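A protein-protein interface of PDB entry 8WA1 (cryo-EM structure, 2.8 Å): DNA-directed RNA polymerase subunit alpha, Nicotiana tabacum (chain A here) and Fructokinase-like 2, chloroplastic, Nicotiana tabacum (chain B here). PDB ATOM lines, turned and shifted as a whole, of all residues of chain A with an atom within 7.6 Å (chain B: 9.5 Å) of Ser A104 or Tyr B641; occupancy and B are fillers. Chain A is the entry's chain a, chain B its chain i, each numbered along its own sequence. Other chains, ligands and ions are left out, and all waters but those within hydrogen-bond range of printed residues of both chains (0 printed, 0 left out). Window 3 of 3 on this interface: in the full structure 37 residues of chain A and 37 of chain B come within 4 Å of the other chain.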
ATOM      1  N   THR A  60      -7.310  -6.948  35.201  1.00  0.00           N
ATOM      2  CA  THR A  60      -6.456  -6.018  34.476  1.00  0.00           C
ATOM      3  C   THR A  60      -5.092  -5.953  35.150  1.00  0.00           C
ATOM      4  O   THR A  60      -5.003  -5.941  36.382  1.00  0.00           O
ATOM      5  CB  THR A  60      -7.088  -4.624  34.407  1.00  0.00           C
ATOM      6  OG1 THR A  60      -6.136  -3.689  33.884  1.00  0.00           O
ATOM      7  CG2 THR A  60      -7.544  -4.167  35.784  1.00  0.00           C
ATOM      8  N   THR A  63       0.960  -4.745  31.155  1.00  0.00           N
ATOM      9  CA  THR A  63       1.425  -5.664  30.128  1.00  0.00           C
ATOM     10  C   THR A  63       2.673  -5.198  29.395  1.00  0.00           C
ATOM     11  O   THR A  63       3.350  -6.030  28.783  1.00  0.00           O
ATOM     12  CB  THR A  63       0.318  -5.913  29.092  1.00  0.00           C
ATOM     13  OG1 THR A  63      -0.060  -4.671  28.487  1.00  0.00           O
ATOM     14  CG2 THR A  63      -0.898  -6.544  29.750  1.00  0.00           C
ATOM     15  N   ARG A  64       2.997  -3.908  29.436  1.00  0.00           N
ATOM     16  CA  ARG A  64       4.155  -3.404  28.716  1.00  0.00           C
ATOM     17  C   ARG A  64       4.756  -2.234  29.480  1.00  0.00           C
ATOM     18  O   ARG A  64       4.028  -1.387  30.006  1.00  0.00           O
ATOM     19  CB  ARG A  64       3.780  -2.979  27.292  1.00  0.00           C
ATOM     20  CG  ARG A  64       4.955  -2.915  26.336  1.00  0.00           C
ATOM     21  CD  ARG A  64       4.485  -2.734  24.904  1.00  0.00           C
ATOM     22  NE  ARG A  64       5.587  -2.822  23.953  1.00  0.00           N
ATOM     23  CZ  ARG A  64       6.005  -3.955  23.397  1.00  0.00           C
ATOM     24  NH1 ARG A  64       7.018  -3.941  22.541  1.00  0.00           N
ATOM     25  NH2 ARG A  64       5.410  -5.101  23.696  1.00  0.00           N
ATOM     26  N   LEU A  96      -4.563  -3.872  39.742  1.00  0.00           N
ATOM     27  CA  LEU A  96      -5.354  -2.774  39.209  1.00  0.00           C
ATOM     28  C   LEU A  96      -6.811  -3.203  39.094  1.00  0.00           C
ATOM     29  O   LEU A  96      -7.135  -4.393  39.127  1.00  0.00           O
ATOM     30  CB  LEU A  96      -4.829  -2.316  37.841  1.00  0.00           C
ATOM     31  CG  LEU A  96      -3.340  -1.970  37.773  1.00  0.00           C
ATOM     32  CD1 LEU A  96      -2.907  -1.733  36.337  1.00  0.00           C
ATOM     33  CD2 LEU A  96      -3.031  -0.759  38.635  1.00  0.00           C
ATOM     34  N   ARG A  97      -7.691  -2.215  38.953  1.00  0.00           N
ATOM     35  CA  ARG A  97      -9.124  -2.445  38.829  1.00  0.00           C
ATOM     36  C   ARG A  97      -9.662  -1.679  37.630  1.00  0.00           C
ATOM     37  O   ARG A  97      -9.476  -0.462  37.530  1.00  0.00           O
ATOM     38  CB  ARG A  97      -9.861  -2.025  40.104  1.00  0.00           C
ATOM     39  CG  ARG A  97     -11.376  -2.133  40.010  1.00  0.00           C
ATOM     40  CD  ARG A  97     -12.045  -1.920  41.364  1.00  0.00           C
ATOM     41  NE  ARG A  97     -11.710  -0.629  41.962  1.00  0.00           N
ATOM     42  CZ  ARG A  97     -10.833  -0.466  42.949  1.00  0.00           C
ATOM     43  NH1 ARG A  97     -10.198  -1.515  43.454  1.00  0.00           N
ATOM     44  NH2 ARG A  97     -10.592   0.745  43.431  1.00  0.00           N
ATOM     45  N   SER A  98     -10.326  -2.395  36.725  1.00  0.00           N
ATOM     46  CA  SER A  98     -10.907  -1.793  35.535  1.00  0.00           C
ATOM     47  C   SER A  98     -12.052  -2.666  35.049  1.00  0.00           C
ATOM     48  O   SER A  98     -12.058  -3.881  35.262  1.00  0.00           O
ATOM     49  CB  SER A  98      -9.864  -1.616  34.425  1.00  0.00           C
ATOM     50  OG  SER A  98     -10.447  -1.053  33.263  1.00  0.00           O
ATOM     51  N   ASN A  99     -13.025  -2.034  34.391  1.00  0.00           N
ATOM     52  CA  ASN A  99     -14.211  -2.728  33.905  1.00  0.00           C
ATOM     53  C   ASN A  99     -14.418  -2.572  32.404  1.00  0.00           C
ATOM     54  O   ASN A  99     -15.478  -2.953  31.893  1.00  0.00           O
ATOM     55  CB  ASN A  99     -15.455  -2.238  34.654  1.00  0.00           C
ATOM     56  CG  ASN A  99     -15.360  -2.459  36.150  1.00  0.00           C
ATOM     57  OD1 ASN A  99     -15.459  -1.516  36.935  1.00  0.00           O
ATOM     58  ND2 ASN A  99     -15.166  -3.709  36.552  1.00  0.00           N
ATOM     59  N   LEU A 100     -13.440  -2.028  31.683  1.00  0.00           N
ATOM     60  CA  LEU A 100     -13.548  -1.836  30.245  1.00  0.00           C
ATOM     61  C   LEU A 100     -12.356  -2.473  29.548  1.00  0.00           C
ATOM     62  O   LEU A 100     -11.237  -2.454  30.070  1.00  0.00           O
ATOM     63  CB  LEU A 100     -13.630  -0.348  29.885  1.00  0.00           C
ATOM     64  CG  LEU A 100     -14.842   0.414  30.421  1.00  0.00           C
ATOM     65  CD1 LEU A 100     -14.821   1.855  29.940  1.00  0.00           C
ATOM     66  CD2 LEU A 100     -16.136  -0.271  30.011  1.00  0.00           C
ATOM     67  N   TYR A 101     -12.602  -3.030  28.367  1.00  0.00           N
ATOM     68  CA  TYR A 101     -11.561  -3.681  27.586  1.00  0.00           C
ATOM     69  C   TYR A 101     -10.798  -2.658  26.751  1.00  0.00           C
ATOM     70  O   TYR A 101     -11.253  -1.534  26.527  1.00  0.00           O
ATOM     71  CB  TYR A 101     -12.159  -4.755  26.677  1.00  0.00           C
ATOM     72  CG  TYR A 101     -12.954  -5.811  27.411  1.00  0.00           C
ATOM     73  CD1 TYR A 101     -12.335  -6.939  27.929  1.00  0.00           C
ATOM     74  CD2 TYR A 101     -14.326  -5.680  27.582  1.00  0.00           C
ATOM     75  CE1 TYR A 101     -13.058  -7.908  28.599  1.00  0.00           C
ATOM     76  CE2 TYR A 101     -15.058  -6.642  28.250  1.00  0.00           C
ATOM     77  CZ  TYR A 101     -14.420  -7.753  28.756  1.00  0.00           C
ATOM     78  OH  TYR A 101     -15.146  -8.712  29.422  1.00  0.00           O
ATOM     79  N   GLY A 102      -9.625  -3.065  26.289  1.00  0.00           N
ATOM     80  CA  GLY A 102      -8.763  -2.219  25.491  1.00  0.00           C
ATOM     81  C   GLY A 102      -7.460  -1.902  26.203  1.00  0.00           C
ATOM     82  O   GLY A 102      -7.234  -2.266  27.354  1.00  0.00           O
ATOM     83  N   THR A 103      -6.597  -1.202  25.474  1.00  0.00           N
ATOM     84  CA  THR A 103      -5.296  -0.792  25.981  1.00  0.00           C
ATOM     85  C   THR A 103      -5.343   0.666  26.418  1.00  0.00           C
ATOM     86  O   THR A 103      -5.886   1.519  25.711  1.00  0.00           O
ATOM     87  CB  THR A 103      -4.211  -0.983  24.920  1.00  0.00           C
ATOM     88  OG1 THR A 103      -4.298  -2.307  24.377  1.00  0.00           O
ATOM     89  CG2 THR A 103      -2.829  -0.787  25.527  1.00  0.00           C
ATOM     90  N   SER A 104      -4.769   0.945  27.587  1.00  0.00           N
ATOM     91  CA  SER A 104      -4.665   2.303  28.099  1.00  0.00           C
ATOM     92  C   SER A 104      -3.213   2.585  28.450  1.00  0.00           C
ATOM     93  O   SER A 104      -2.389   1.673  28.550  1.00  0.00           O
ATOM     94  CB  SER A 104      -5.564   2.528  29.322  1.00  0.00           C
ATOM     95  OG  SER A 104      -5.072   1.834  30.456  1.00  0.00           O
ATOM     96  N   ASP A 105      -2.906   3.866  28.643  1.00  0.00           N
ATOM     97  CA  ASP A 105      -1.541   4.314  28.871  1.00  0.00           C
ATOM     98  C   ASP A 105      -1.415   4.936  30.255  1.00  0.00           C
ATOM     99  O   ASP A 105      -2.286   5.697  30.686  1.00  0.00           O
ATOM    100  CB  ASP A 105      -1.105   5.325  27.805  1.00  0.00           C
ATOM    101  CG  ASP A 105      -1.191   4.762  26.400  1.00  0.00           C
ATOM    102  OD1 ASP A 105      -2.319   4.499  25.933  1.00  0.00           O
ATOM    103  OD2 ASP A 105      -0.132   4.583  25.763  1.00  0.00           O
ATOM    104  N   ALA A 106      -0.324   4.604  30.942  1.00  0.00           N
ATOM    105  CA  ALA A 106      -0.001   5.178  32.239  1.00  0.00           C
ATOM    106  C   ALA A 106       1.467   5.585  32.229  1.00  0.00           C
ATOM    107  O   ALA A 106       2.209   5.288  31.288  1.00  0.00           O
ATOM    108  CB  ALA A 106      -0.302   4.196  33.377  1.00  0.00           C
ATOM    109  N   LEU A 123      -2.995   7.359  36.433  1.00  0.00           N
ATOM    110  CA  LEU A 123      -3.849   6.409  35.740  1.00  0.00           C
ATOM    111  C   LEU A 123      -4.931   7.135  34.962  1.00  0.00           C
ATOM    112  O   LEU A 123      -5.290   8.271  35.288  1.00  0.00           O
ATOM    113  CB  LEU A 123      -4.504   5.438  36.735  1.00  0.00           C
ATOM    114  CG  LEU A 123      -3.577   4.547  37.559  1.00  0.00           C
ATOM    115  CD1 LEU A 123      -4.379   3.759  38.574  1.00  0.00           C
ATOM    116  CD2 LEU A 123      -2.798   3.615  36.652  1.00  0.00           C
ATOM    117  N   PRO A 124      -5.470   6.504  33.922  1.00  0.00           N
ATOM    118  CA  PRO A 124      -6.679   7.023  33.281  1.00  0.00           C
ATOM    119  C   PRO A 124      -7.841   7.014  34.256  1.00  0.00           C
ATOM    120  O   PRO A 124      -7.787   6.330  35.291  1.00  0.00           O
ATOM    121  CB  PRO A 124      -6.910   6.042  32.121  1.00  0.00           C
ATOM    122  CG  PRO A 124      -5.567   5.454  31.851  1.00  0.00           C
ATOM    123  CD  PRO A 124      -4.903   5.359  33.191  1.00  0.00           C
ATOM    124  N   PRO A 125      -8.914   7.760  33.970  1.00  0.00           N
ATOM    125  CA  PRO A 125     -10.035   7.803  34.926  1.00  0.00           C
ATOM    126  C   PRO A 125     -10.689   6.452  35.159  1.00  0.00           C
ATOM    127  O   PRO A 125     -11.266   6.226  36.230  1.00  0.00           O
ATOM    128  CB  PRO A 125     -11.004   8.805  34.278  1.00  0.00           C
ATOM    129  CG  PRO A 125     -10.637   8.811  32.830  1.00  0.00           C
ATOM    130  CD  PRO A 125      -9.156   8.611  32.795  1.00  0.00           C
ATOM    131  N   TYR A 126     -10.621   5.545  34.183  1.00  0.00           N
ATOM    132  CA  TYR A 126     -11.277   4.250  34.332  1.00  0.00           C
ATOM    133  C   TYR A 126     -10.476   3.311  35.226  1.00  0.00           C
ATOM    134  O   TYR A 126     -11.056   2.542  36.002  1.00  0.00           O
ATOM    135  CB  TYR A 126     -11.508   3.619  32.961  1.00  0.00           C
ATOM    136  CG  TYR A 126     -12.410   4.437  32.066  1.00  0.00           C
ATOM    137  CD1 TYR A 126     -13.788   4.422  32.239  1.00  0.00           C
ATOM    138  CD2 TYR A 126     -11.886   5.225  31.050  1.00  0.00           C
ATOM    139  CE1 TYR A 126     -14.619   5.167  31.426  1.00  0.00           C
ATOM    140  CE2 TYR A 126     -12.709   5.975  30.231  1.00  0.00           C
ATOM    141  CZ  TYR A 126     -14.074   5.942  30.424  1.00  0.00           C
ATOM    142  OH  TYR A 126     -14.897   6.687  29.610  1.00  0.00           O
ATOM    143  N   VAL A 127      -9.148   3.343  35.124  1.00  0.00           N
ATOM    144  CA  VAL A 127      -8.315   2.442  35.911  1.00  0.00           C
ATOM    145  C   VAL A 127      -8.063   3.038  37.294  1.00  0.00           C
ATOM    146  O   VAL A 127      -7.977   4.256  37.474  1.00  0.00           O
ATOM    147  CB  VAL A 127      -6.993   2.142  35.180  1.00  0.00           C
ATOM    148  CG1 VAL A 127      -6.281   0.956  35.815  1.00  0.00           C
ATOM    149  CG2 VAL A 127      -7.253   1.887  33.704  1.00  0.00           C
ATOM    150  N   LEU A 149       3.800   2.920  30.972  1.00  0.00           N
ATOM    151  CA  LEU A 149       3.103   1.676  31.266  1.00  0.00           C
ATOM    152  C   LEU A 149       1.880   1.543  30.373  1.00  0.00           C
ATOM    153  O   LEU A 149       1.171   2.523  30.129  1.00  0.00           O
ATOM    154  CB  LEU A 149       2.676   1.610  32.738  1.00  0.00           C
ATOM    155  CG  LEU A 149       3.773   1.780  33.791  1.00  0.00           C
ATOM    156  CD1 LEU A 149       3.174   1.841  35.186  1.00  0.00           C
ATOM    157  CD2 LEU A 149       4.788   0.655  33.693  1.00  0.00           C
ATOM    158  N   GLN A 150       1.640   0.327  29.890  1.00  0.00           N
ATOM    159  CA  GLN A 150       0.438  -0.005  29.138  1.00  0.00           C
ATOM    160  C   GLN A 150      -0.410  -0.967  29.956  1.00  0.00           C
ATOM    161  O   GLN A 150       0.084  -2.002  30.413  1.00  0.00           O
ATOM    162  CB  GLN A 150       0.783  -0.622  27.781  1.00  0.00           C
ATOM    163  CG  GLN A 150       1.384   0.355  26.786  1.00  0.00           C
ATOM    164  CD  GLN A 150       1.467  -0.221  25.387  1.00  0.00           C
ATOM    165  OE1 GLN A 150       1.265  -1.417  25.183  1.00  0.00           O
ATOM    166  NE2 GLN A 150       1.760   0.633  24.412  1.00  0.00           N
ATOM    167  N   ILE A 151      -1.682  -0.623  30.140  1.00  0.00           N
ATOM    168  CA  ILE A 151      -2.604  -1.396  30.962  1.00  0.00           C
ATOM    169  C   ILE A 151      -3.641  -2.041  30.052  1.00  0.00           C
ATOM    170  O   ILE A 151      -4.266  -1.359  29.232  1.00  0.00           O
ATOM    171  CB  ILE A 151      -3.276  -0.515  32.028  1.00  0.00           C
ATOM    172  CG1 ILE A 151      -2.215   0.199  32.866  1.00  0.00           C
ATOM    173  CG2 ILE A 151      -4.180  -1.349  32.915  1.00  0.00           C
ATOM    174  CD1 ILE A 151      -2.787   1.119  33.919  1.00  0.00           C
ATOM    175  N   GLU A 152      -3.821  -3.351  30.199  1.00  0.00           N
ATOM    176  CA  GLU A 152      -4.764  -4.103  29.386  1.00  0.00           C
ATOM    177  C   GLU A 152      -5.578  -5.021  30.287  1.00  0.00           C
ATOM    178  O   GLU A 152      -5.136  -5.414  31.369  1.00  0.00           O
ATOM    179  CB  GLU A 152      -4.041  -4.913  28.298  1.00  0.00           C
ATOM    180  CG  GLU A 152      -4.946  -5.476  27.212  1.00  0.00           C
ATOM    181  CD  GLU A 152      -4.187  -6.302  26.191  1.00  0.00           C
ATOM    182  OE1 GLU A 152      -2.977  -6.537  26.395  1.00  0.00           O
ATOM    183  OE2 GLU A 152      -4.798  -6.714  25.183  1.00  0.00           O
ATOM    184  N   ARG A 153      -6.779  -5.364  29.824  1.00  0.00           N
ATOM    185  CA  ARG A 153      -7.687  -6.248  30.544  1.00  0.00           C
ATOM    186  C   ARG A 153      -7.915  -7.500  29.711  1.00  0.00           C
ATOM    187  O   ARG A 153      -8.406  -7.416  28.581  1.00  0.00           O
ATOM    188  CB  ARG A 153      -9.017  -5.552  30.841  1.00  0.00           C
ATOM    189  CG  ARG A 153     -10.069  -6.463  31.456  1.00  0.00           C
ATOM    190  CD  ARG A 153     -11.377  -5.725  31.688  1.00  0.00           C
ATOM    191  NE  ARG A 153     -12.435  -6.617  32.151  1.00  0.00           N
ATOM    192  CZ  ARG A 153     -12.706  -6.856  33.430  1.00  0.00           C
ATOM    193  NH1 ARG A 153     -11.995  -6.268  34.382  1.00  0.00           N
ATOM    194  NH2 ARG A 153     -13.690  -7.683  33.758  1.00  0.00           N
ATOM    195  N   ASP B 311     -19.996   2.549  34.425  1.00  0.00           N
ATOM    196  CA  ASP B 311     -19.505   2.814  33.075  1.00  0.00           C
ATOM    197  C   ASP B 311     -19.763   1.632  32.148  1.00  0.00           C
ATOM    198  O   ASP B 311     -20.181   1.808  30.999  1.00  0.00           O
ATOM    199  CB  ASP B 311     -18.013   3.151  33.123  1.00  0.00           C
ATOM    200  CG  ASP B 311     -17.206   2.120  33.890  1.00  0.00           C
ATOM    201  OD1 ASP B 311     -17.005   1.009  33.359  1.00  0.00           O
ATOM    202  OD2 ASP B 311     -16.775   2.420  35.023  1.00  0.00           O
ATOM    203  N   ALA B 312     -19.515   0.413  32.633  1.00  0.00           N
ATOM    204  CA  ALA B 312     -19.631  -0.760  31.773  1.00  0.00           C
ATOM    205  C   ALA B 312     -21.087  -1.142  31.535  1.00  0.00           C
ATOM    206  O   ALA B 312     -21.512  -1.304  30.385  1.00  0.00           O
ATOM    207  CB  ALA B 312     -18.862  -1.933  32.380  1.00  0.00           C
ATOM    208  N   LYS B 619     -21.263   2.461  20.202  1.00  0.00           N
ATOM    209  CA  LYS B 619     -20.917   3.562  21.093  1.00  0.00           C
ATOM    210  C   LYS B 619     -20.546   4.801  20.285  1.00  0.00           C
ATOM    211  O   LYS B 619     -20.766   4.842  19.070  1.00  0.00           O
ATOM    212  CB  LYS B 619     -19.776   3.158  22.031  1.00  0.00           C
ATOM    213  CG  LYS B 619     -19.953   3.663  23.450  1.00  0.00           C
ATOM    214  CD  LYS B 619     -18.919   3.066  24.392  1.00  0.00           C
ATOM    215  CE  LYS B 619     -19.155   3.538  25.818  1.00  0.00           C
ATOM    216  NZ  LYS B 619     -18.164   2.969  26.772  1.00  0.00           N
ATOM    217  N   GLU B 620     -19.993   5.814  20.957  1.00  0.00           N
ATOM    218  CA  GLU B 620     -19.668   7.071  20.285  1.00  0.00           C
ATOM    219  C   GLU B 620     -18.783   6.840  19.065  1.00  0.00           C
ATOM    220  O   GLU B 620     -18.921   7.531  18.048  1.00  0.00           O
ATOM    221  CB  GLU B 620     -18.989   8.027  21.268  1.00  0.00           C
ATOM    222  CG  GLU B 620     -19.733   8.186  22.589  1.00  0.00           C
ATOM    223  CD  GLU B 620     -21.081   8.860  22.425  1.00  0.00           C
ATOM    224  OE1 GLU B 620     -21.261   9.608  21.441  1.00  0.00           O
ATOM    225  OE2 GLU B 620     -21.964   8.642  23.282  1.00  0.00           O
ATOM    226  N   GLY B 621     -17.870   5.876  19.147  1.00  0.00           N
ATOM    227  CA  GLY B 621     -17.082   5.490  17.994  1.00  0.00           C
ATOM    228  C   GLY B 621     -17.692   4.316  17.258  1.00  0.00           C
ATOM    229  O   GLY B 621     -17.502   3.162  17.655  1.00  0.00           O
ATOM    230  N   VAL B 636     -18.846  -7.322  24.629  1.00  0.00           N
ATOM    231  CA  VAL B 636     -17.410  -7.072  24.725  1.00  0.00           C
ATOM    232  C   VAL B 636     -17.023  -5.875  23.866  1.00  0.00           C
ATOM    233  O   VAL B 636     -16.187  -5.053  24.260  1.00  0.00           O
ATOM    234  CB  VAL B 636     -16.620  -8.333  24.330  1.00  0.00           C
ATOM    235  CG1 VAL B 636     -15.131  -8.124  24.564  1.00  0.00           C
ATOM    236  CG2 VAL B 636     -17.126  -9.539  25.105  1.00  0.00           C
ATOM    237  N   THR B 637     -17.624  -5.757  22.680  1.00  0.00           N
ATOM    238  CA  THR B 637     -17.313  -4.634  21.800  1.00  0.00           C
ATOM    239  C   THR B 637     -17.794  -3.317  22.395  1.00  0.00           C
ATOM    240  O   THR B 637     -17.146  -2.278  22.223  1.00  0.00           O
ATOM    241  CB  THR B 637     -17.936  -4.862  20.422  1.00  0.00           C
ATOM    242  OG1 THR B 637     -17.539  -6.145  19.924  1.00  0.00           O
ATOM    243  CG2 THR B 637     -17.478  -3.788  19.443  1.00  0.00           C
ATOM    244  N   GLU B 638     -18.928  -3.336  23.099  1.00  0.00           N
ATOM    245  CA  GLU B 638     -19.455  -2.103  23.672  1.00  0.00           C
ATOM    246  C   GLU B 638     -18.616  -1.639  24.858  1.00  0.00           C
ATOM    247  O   GLU B 638     -18.527  -0.436  25.131  1.00  0.00           O
ATOM    248  CB  GLU B 638     -20.914  -2.298  24.087  1.00  0.00           C
ATOM    249  CG  GLU B 638     -21.673  -1.000  24.308  1.00  0.00           C
ATOM    250  CD  GLU B 638     -22.161  -0.841  25.732  1.00  0.00           C
ATOM    251  OE1 GLU B 638     -21.804  -1.683  26.583  1.00  0.00           O
ATOM    252  OE2 GLU B 638     -22.905   0.125  26.004  1.00  0.00           O
ATOM    253  N   ARG B 639     -17.994  -2.575  25.572  1.00  0.00           N
ATOM    254  CA  ARG B 639     -17.196  -2.245  26.754  1.00  0.00           C
ATOM    255  C   ARG B 639     -15.751  -1.923  26.365  1.00  0.00           C
ATOM    256  O   ARG B 639     -14.805  -2.632  26.708  1.00  0.00           O
ATOM    257  CB  ARG B 639     -17.255  -3.384  27.766  1.00  0.00           C
ATOM    258  CG  ARG B 639     -18.612  -3.571  28.418  1.00  0.00           C
ATOM    259  CD  ARG B 639     -18.553  -4.629  29.506  1.00  0.00           C
ATOM    260  NE  ARG B 639     -19.845  -4.814  30.158  1.00  0.00           N
ATOM    261  CZ  ARG B 639     -20.075  -5.693  31.127  1.00  0.00           C
ATOM    262  NH1 ARG B 639     -19.096  -6.473  31.565  1.00  0.00           N
ATOM    263  NH2 ARG B 639     -21.284  -5.792  31.660  1.00  0.00           N
ATOM    264  N   GLU B 640     -15.593  -0.824  25.633  1.00  0.00           N
ATOM    265  CA  GLU B 640     -14.284  -0.318  25.248  1.00  0.00           C
ATOM    266  C   GLU B 640     -13.983   0.979  25.987  1.00  0.00           C
ATOM    267  O   GLU B 640     -14.872   1.624  26.550  1.00  0.00           O
ATOM    268  CB  GLU B 640     -14.199  -0.092  23.735  1.00  0.00           C
ATOM    269  CG  GLU B 640     -14.219  -1.368  22.910  1.00  0.00           C
ATOM    270  CD  GLU B 640     -12.982  -2.223  23.109  1.00  0.00           C
ATOM    271  OE1 GLU B 640     -11.943  -1.682  23.543  1.00  0.00           O
ATOM    272  OE2 GLU B 640     -13.048  -3.439  22.832  1.00  0.00           O
ATOM    273  N   TYR B 641     -12.700   1.350  25.986  1.00  0.00           N
ATOM    274  CA  TYR B 641     -12.283   2.574  26.662  1.00  0.00           C
ATOM    275  C   TYR B 641     -12.869   3.809  25.991  1.00  0.00           C
ATOM    276  O   TYR B 641     -13.324   4.737  26.672  1.00  0.00           O
ATOM    277  CB  TYR B 641     -10.757   2.655  26.704  1.00  0.00           C
ATOM    278  CG  TYR B 641     -10.133   1.823  27.802  1.00  0.00           C
ATOM    279  CD1 TYR B 641     -10.756   1.688  29.036  1.00  0.00           C
ATOM    280  CD2 TYR B 641      -8.918   1.181  27.608  1.00  0.00           C
ATOM    281  CE1 TYR B 641     -10.189   0.931  30.044  1.00  0.00           C
ATOM    282  CE2 TYR B 641      -8.343   0.422  28.610  1.00  0.00           C
ATOM    283  CZ  TYR B 641      -8.983   0.301  29.826  1.00  0.00           C
ATOM    284  OH  TYR B 641      -8.414  -0.453  30.827  1.00  0.00           O
ATOM    285  N   ARG B 642     -12.867   3.845  24.663  1.00  0.00           N
ATOM    286  CA  ARG B 642     -13.424   4.978  23.934  1.00  0.00           C
ATOM    287  C   ARG B 642     -14.265   4.507  22.754  1.00  0.00           C
ATOM    288  O   ARG B 642     -14.562   3.319  22.625  1.00  0.00           O
ATOM    289  CB  ARG B 642     -12.309   5.906  23.449  1.00  0.00           C
ATOM    290  CG  ARG B 642     -11.408   5.295  22.390  1.00  0.00           C
ATOM    291  CD  ARG B 642     -10.317   6.264  21.965  1.00  0.00           C
ATOM    292  NE  ARG B 642      -9.485   5.716  20.898  1.00  0.00           N
ATOM    293  CZ  ARG B 642      -8.414   4.955  21.101  1.00  0.00           C
ATOM    294  NH1 ARG B 642      -7.716   4.501  20.070  1.00  0.00           N
ATOM    295  NH2 ARG B 642      -8.042   4.646  22.336  1.00  0.00           N
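The side-chain hydroxyl of Ser A98 is in hydrogen-bond range of the side-chain hydroxyl of Tyr B641, 3.2 Å away.
N of Tyr A101 lies within hydrogen-bond range of O of Arg B639 (2.8 Å).
The backbone NH (N) of Tyr B641 sits at hydrogen-bond distance from the backbone carbonyl oxygen (O) of Tyr A101 (3.3 Å).
The backbone carbonyl oxygen of Tyr A101 sits close to the side-chain carboxylate of Glu B640 (3.1 Å).
The guanidinium group (NH1) of Arg A153 is in hydrogen-bond range of the backbone carbonyl oxygen (O) of Ser A98.
N of Ser A104 sits at hydrogen-bond distance from O of Ile A151.
Among the printed residues, merely in contact across the chains: Gly A102 with Tyr B641 (3.2 Å), Leu A100 with Glu B640 (3.4 Å), Leu A100 with Tyr B641 (3.5 Å), Ser A104 with Tyr B641 (3.6 Å), Asn A99 with Ala B312 (3.6 Å), Thr A103 with Tyr B641 (3.6 Å), Leu A100 with Asp B311 (3.7 Å), Leu A100 with Arg B639 (3.8 Å), Gly A102 with Glu B640 (3.8 Å), Tyr A126 with Tyr B641 (3.8 Å), Asn A99 with Asp B311 (3.8 Å), Tyr A101 with Val B636 (3.9 Å), Val A127 with Tyr B641 (3.9 Å) and Leu A100 with Ala B312 (3.9 Å).
Ser A104 touches just one residue of chain B: Tyr B641 (3.6 Å).
Of chain A, only Ser A98 (3.2 Å), Leu A100 (3.5 Å), Tyr A101 (3.3 Å), Gly A102 (3.2 Å), Thr A103 (3.6 Å), Ser A104 (3.6 Å), Tyr A126 (3.8 Å) and Val A127 (3.9 Å) come within 4 Å of Tyr B641.
Of chain B, only Glu B640 and Tyr B641 come within 4 Å of Gly A102.
Of chain B, only Tyr B641 (3.6 Å) comes within 4 Å of Thr A103.
No residue of chain B comes within 4 Å of Asp A105.
Ile A151 touches none of the printed residues of chain B.
Of the printed residues of chain B, Val A127 touches Tyr B641.
Printed residues of chain B within 4 Å of Leu A100: Asp B311 (3.7 Å), Ala B312 (3.9 Å), Arg B639 (3.8 Å), Glu B640 (3.4 Å) and Tyr B641 (3.5 Å).
Leu A123 touches none of the printed residues of chain B.
The nearest residue of chain A that does not touch Tyr B641 is Ile A151 (4.5 Å).
Of the 24 printed residues of chain A, 9 touch a printed residue of chain B.
Hydrophobic or aromatic side chains of chain B that line the printed part of chain A: Ala B312, Val B636 and Tyr B641.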
